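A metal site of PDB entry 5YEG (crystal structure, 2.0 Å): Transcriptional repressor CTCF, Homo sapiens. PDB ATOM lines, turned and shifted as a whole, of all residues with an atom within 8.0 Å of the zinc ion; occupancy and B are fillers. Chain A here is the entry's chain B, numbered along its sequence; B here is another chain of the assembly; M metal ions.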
ATOM      1  N   GLN A  32     -19.449  -9.631 -15.717  1.00  0.00           N
ATOM      2  CA  GLN A  32     -20.396  -9.803 -16.807  1.00  0.00           C
ATOM      3  C   GLN A  32     -19.908 -10.880 -17.765  1.00  0.00           C
ATOM      4  O   GLN A  32     -18.735 -10.916 -18.137  1.00  0.00           O
ATOM      5  CB  GLN A  32     -20.594  -8.478 -17.545  1.00  0.00           C
ATOM      6  CG  GLN A  32     -21.420  -8.577 -18.821  1.00  0.00           C
ATOM      7  CD  GLN A  32     -22.875  -8.874 -18.558  1.00  0.00           C
ATOM      8  OE1 GLN A  32     -23.527  -8.183 -17.765  1.00  0.00           O
ATOM      9  NE2 GLN A  32     -23.411  -9.896 -19.211  1.00  0.00           N
ATOM     10  N   CYS A  33     -20.814 -11.762 -18.172  1.00  0.00           N
ATOM     11  CA  CYS A  33     -20.449 -12.734 -19.192  1.00  0.00           C
ATOM     12  C   CYS A  33     -20.290 -12.029 -20.529  1.00  0.00           C
ATOM     13  O   CYS A  33     -21.122 -11.200 -20.913  1.00  0.00           O
ATOM     14  CB  CYS A  33     -21.507 -13.836 -19.279  1.00  0.00           C
ATOM     15  SG  CYS A  33     -21.149 -14.996 -20.581  1.00  0.00           S
ATOM     16  N   SER A  34     -19.209 -12.359 -21.258  1.00  0.00           N
ATOM     17  CA  SER A  34     -18.999 -11.758 -22.572  1.00  0.00           C
ATOM     18  C   SER A  34     -19.886 -12.352 -23.651  1.00  0.00           C
ATOM     19  O   SER A  34     -19.944 -11.803 -24.759  1.00  0.00           O
ATOM     20  CB  SER A  34     -17.529 -11.895 -22.998  1.00  0.00           C
ATOM     21  OG  SER A  34     -17.147 -13.264 -22.983  1.00  0.00           O
ATOM     22  N   LEU A  35     -20.572 -13.453 -23.357  1.00  0.00           N
ATOM     23  CA  LEU A  35     -21.321 -14.178 -24.367  1.00  0.00           C
ATOM     24  C   LEU A  35     -22.834 -14.083 -24.200  1.00  0.00           C
ATOM     25  O   LEU A  35     -23.551 -14.410 -25.157  1.00  0.00           O
ATOM     26  CB  LEU A  35     -20.914 -15.666 -24.364  1.00  0.00           C
ATOM     27  CG  LEU A  35     -19.422 -15.932 -24.586  1.00  0.00           C
ATOM     28  CD1 LEU A  35     -19.123 -17.414 -24.723  1.00  0.00           C
ATOM     29  CD2 LEU A  35     -18.862 -15.155 -25.778  1.00  0.00           C
ATOM     30  N   CYS A  36     -23.338 -13.751 -23.023  1.00  0.00           N
ATOM     31  CA  CYS A  36     -24.779 -13.587 -22.832  1.00  0.00           C
ATOM     32  C   CYS A  36     -25.009 -12.503 -21.775  1.00  0.00           C
ATOM     33  O   CYS A  36     -24.065 -11.822 -21.360  1.00  0.00           O
ATOM     34  CB  CYS A  36     -25.433 -14.929 -22.470  1.00  0.00           C
ATOM     35  SG  CYS A  36     -25.243 -15.440 -20.740  1.00  0.00           S
ATOM     36  N   SER A  37     -26.253 -12.352 -21.335  1.00  0.00           N
ATOM     37  CA  SER A  37     -26.561 -11.268 -20.406  1.00  0.00           C
ATOM     38  C   SER A  37     -26.299 -11.614 -18.937  1.00  0.00           C
ATOM     39  O   SER A  37     -26.421 -10.723 -18.088  1.00  0.00           O
ATOM     40  CB  SER A  37     -28.017 -10.806 -20.561  1.00  0.00           C
ATOM     41  OG  SER A  37     -28.915 -11.774 -20.068  1.00  0.00           O
ATOM     42  N   TYR A  38     -25.965 -12.871 -18.626  1.00  0.00           N
ATOM     43  CA  TYR A  38     -25.689 -13.252 -17.244  1.00  0.00           C
ATOM     44  C   TYR A  38     -24.525 -12.435 -16.670  1.00  0.00           C
ATOM     45  O   TYR A  38     -23.537 -12.179 -17.355  1.00  0.00           O
ATOM     46  CB  TYR A  38     -25.369 -14.749 -17.140  1.00  0.00           C
ATOM     47  CG  TYR A  38     -24.935 -15.132 -15.759  1.00  0.00           C
ATOM     48  CD1 TYR A  38     -25.855 -15.187 -14.711  1.00  0.00           C
ATOM     49  CD2 TYR A  38     -23.608 -15.390 -15.459  1.00  0.00           C
ATOM     50  CE1 TYR A  38     -25.459 -15.508 -13.431  1.00  0.00           C
ATOM     51  CE2 TYR A  38     -23.204 -15.725 -14.191  1.00  0.00           C
ATOM     52  CZ  TYR A  38     -24.130 -15.784 -13.177  1.00  0.00           C
ATOM     53  OH  TYR A  38     -23.712 -16.108 -11.895  1.00  0.00           O
ATOM     54  N   ALA A  39     -24.644 -12.055 -15.401  1.00  0.00           N
ATOM     55  CA  ALA A  39     -23.565 -11.429 -14.648  1.00  0.00           C
ATOM     56  C   ALA A  39     -23.557 -11.950 -13.214  1.00  0.00           C
ATOM     57  O   ALA A  39     -24.617 -12.219 -12.638  1.00  0.00           O
ATOM     58  CB  ALA A  39     -23.687  -9.885 -14.642  1.00  0.00           C
ATOM     59  N   LEU A  46     -19.168 -16.653 -12.379  1.00  0.00           N
ATOM     60  CA  LEU A  46     -19.017 -16.373 -13.804  1.00  0.00           C
ATOM     61  C   LEU A  46     -18.207 -17.456 -14.497  1.00  0.00           C
ATOM     62  O   LEU A  46     -18.605 -17.978 -15.553  1.00  0.00           O
ATOM     63  CB  LEU A  46     -18.382 -14.991 -14.020  1.00  0.00           C
ATOM     64  CG  LEU A  46     -18.205 -14.654 -15.511  1.00  0.00           C
ATOM     65  CD1 LEU A  46     -19.575 -14.624 -16.192  1.00  0.00           C
ATOM     66  CD2 LEU A  46     -17.474 -13.334 -15.754  1.00  0.00           C
ATOM     67  N   HIS A  49     -20.196 -20.445 -14.799  1.00  0.00           N
ATOM     68  CA  HIS A  49     -21.200 -20.179 -15.814  1.00  0.00           C
ATOM     69  C   HIS A  49     -20.673 -20.412 -17.227  1.00  0.00           C
ATOM     70  O   HIS A  49     -21.454 -20.776 -18.120  1.00  0.00           O
ATOM     71  CB  HIS A  49     -21.700 -18.734 -15.681  1.00  0.00           C
ATOM     72  CG  HIS A  49     -22.488 -18.277 -16.863  1.00  0.00           C
ATOM     73  ND1 HIS A  49     -23.781 -18.689 -17.101  1.00  0.00           N
ATOM     74  CD2 HIS A  49     -22.163 -17.441 -17.888  1.00  0.00           C
ATOM     75  CE1 HIS A  49     -24.227 -18.129 -18.202  1.00  0.00           C
ATOM     76  NE2 HIS A  49     -23.272 -17.367 -18.702  1.00  0.00           N
ATOM     77  N   MET A  50     -19.393 -20.122 -17.475  1.00  0.00           N
ATOM     78  CA  MET A  50     -18.870 -20.257 -18.836  1.00  0.00           C
ATOM     79  C   MET A  50     -18.941 -21.700 -19.329  1.00  0.00           C
ATOM     80  O   MET A  50     -18.953 -21.952 -20.555  1.00  0.00           O
ATOM     81  CB  MET A  50     -17.431 -19.739 -18.889  1.00  0.00           C
ATOM     82  CG  MET A  50     -17.289 -18.268 -18.496  1.00  0.00           C
ATOM     83  SD  MET A  50     -18.486 -17.187 -19.296  1.00  0.00           S
ATOM     84  CE  MET A  50     -18.014 -17.361 -21.027  1.00  0.00           C
ATOM     85  N   ARG A  51     -19.012 -22.658 -18.401  1.00  0.00           N
ATOM     86  CA  ARG A  51     -19.195 -24.063 -18.766  1.00  0.00           C
ATOM     87  C   ARG A  51     -20.482 -24.267 -19.574  1.00  0.00           C
ATOM     88  O   ARG A  51     -20.535 -25.161 -20.431  1.00  0.00           O
ATOM     89  CB  ARG A  51     -19.228 -24.937 -17.513  1.00  0.00           C
ATOM     90  CG  ARG A  51     -17.999 -24.825 -16.623  1.00  0.00           C
ATOM     91  CD  ARG A  51     -18.036 -25.863 -15.471  1.00  0.00           C
ATOM     92  NE  ARG A  51     -17.083 -25.498 -14.433  1.00  0.00           N
ATOM     93  CZ  ARG A  51     -17.146 -25.914 -13.178  1.00  0.00           C
ATOM     94  NH1 ARG A  51     -18.119 -26.758 -12.818  1.00  0.00           N
ATOM     95  NH2 ARG A  51     -16.236 -25.522 -12.290  1.00  0.00           N
ATOM     96  N   THR A  52     -21.499 -23.446 -19.328  1.00  0.00           N
ATOM     97  CA  THR A  52     -22.756 -23.593 -20.060  1.00  0.00           C
ATOM     98  C   THR A  52     -22.600 -23.214 -21.529  1.00  0.00           C
ATOM     99  O   THR A  52     -23.321 -23.750 -22.380  1.00  0.00           O
ATOM    100  CB  THR A  52     -23.855 -22.746 -19.440  1.00  0.00           C
ATOM    101  OG1 THR A  52     -23.587 -21.352 -19.671  1.00  0.00           O
ATOM    102  CG2 THR A  52     -23.941 -23.010 -17.917  1.00  0.00           C
ATOM    103  N   HIS A  53     -21.672 -22.323 -21.839  1.00  0.00           N
ATOM    104  CA  HIS A  53     -21.454 -21.990 -23.243  1.00  0.00           C
ATOM    105  C   HIS A  53     -20.577 -23.009 -23.945  1.00  0.00           C
ATOM    106  O   HIS A  53     -20.850 -23.369 -25.100  1.00  0.00           O
ATOM    107  CB  HIS A  53     -20.826 -20.602 -23.369  1.00  0.00           C
ATOM    108  CG  HIS A  53     -21.745 -19.492 -22.980  1.00  0.00           C
ATOM    109  ND1 HIS A  53     -22.841 -19.141 -23.734  1.00  0.00           N
ATOM    110  CD2 HIS A  53     -21.747 -18.669 -21.907  1.00  0.00           C
ATOM    111  CE1 HIS A  53     -23.470 -18.145 -23.147  1.00  0.00           C
ATOM    112  NE2 HIS A  53     -22.837 -17.842 -22.033  1.00  0.00           N
ATOM    113  P    DA B  13     -25.227 -21.018 -14.490  1.00  0.00           P
ATOM    114  OP1  DA B  13     -25.293 -20.398 -15.826  1.00  0.00           O
ATOM    115  OP2  DA B  13     -23.934 -21.534 -14.012  1.00  0.00           O
ATOM    116  O5'  DA B  13     -25.683 -20.032 -13.348  1.00  0.00           O
ATOM    117  C5'  DA B  13     -26.985 -19.432 -13.397  1.00  0.00           C
ATOM    118  C4'  DA B  13     -27.433 -19.261 -11.972  1.00  0.00           C
ATOM    119  O4'  DA B  13     -27.493 -20.566 -11.348  1.00  0.00           O
ATOM    120  C3'  DA B  13     -26.485 -18.415 -11.129  1.00  0.00           C
ATOM    121  O3'  DA B  13     -27.236 -17.476 -10.410  1.00  0.00           O
ATOM    122  C2'  DA B  13     -25.810 -19.431 -10.228  1.00  0.00           C
ATOM    123  C1'  DA B  13     -26.872 -20.522 -10.108  1.00  0.00           C
ATOM    124  N9   DA B  13     -26.253 -21.831  -9.849  1.00  0.00           N
ATOM    125  C8   DA B  13     -25.349 -22.490 -10.647  1.00  0.00           C
ATOM    126  N7   DA B  13     -24.911 -23.617 -10.136  1.00  0.00           N
ATOM    127  C5   DA B  13     -25.557 -23.713  -8.922  1.00  0.00           C
ATOM    128  C6   DA B  13     -25.498 -24.668  -7.882  1.00  0.00           C
ATOM    129  N6   DA B  13     -24.733 -25.766  -7.953  1.00  0.00           N
ATOM    130  N1   DA B  13     -26.259 -24.458  -6.788  1.00  0.00           N
ATOM    131  C2   DA B  13     -27.017 -23.353  -6.738  1.00  0.00           C
ATOM    132  N3   DA B  13     -27.145 -22.370  -7.637  1.00  0.00           N
ATOM    133  C4   DA B  13     -26.374 -22.605  -8.712  1.00  0.00           C
HETATM  134 ZN    ZN M   1     -23.010 -16.337 -20.589  1.00  0.00          ZN
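The zinc ion is bound by a ring nitrogen (NE2) of His 53 (2.1 Å).
A ring nitrogen (NE2) of His 49 is bound to the zinc ion (2.2 Å).
The side-chain sulfur (SG) of Cys 33 binds the zinc ion (2.3 Å).
The side-chain sulfur (SG) of Cys 36 binds the zinc ion.
Of the 15 residues printed, 4 come within 4 Å of the zinc ion.
The backbone carbonyl oxygen of His 49 lies within hydrogen-bond range of the side-chain hydroxyl of Thr 52 (2.7 Å).
OP1 of DA 13 of chain B sits at hydrogen-bond distance from a ring nitrogen (ND1) of His 49 (2.6 Å).
The side-chain sulfur (SG) of Cys 33 lies close to the backbone NH (N) of Leu 35 (3.2 Å).
The backbone carbonyl oxygen (O) of Tyr 38 sits at hydrogen-bond distance from the backbone NH (N) of Cys 33, 2.9 Å away.
The side-chain sulfur of Met 50 lies close to the side-chain sulfur of Cys 33, 3.7 Å away.
The side-chain sulfur of Cys 36 lies close to the backbone NH of Tyr 38, at 3.4 Å.
The backbone carbonyl oxygen (O) of Cys 36 is in hydrogen-bond range of the side-chain amide nitrogen (NE2) of Gln 32 (3.0 Å).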
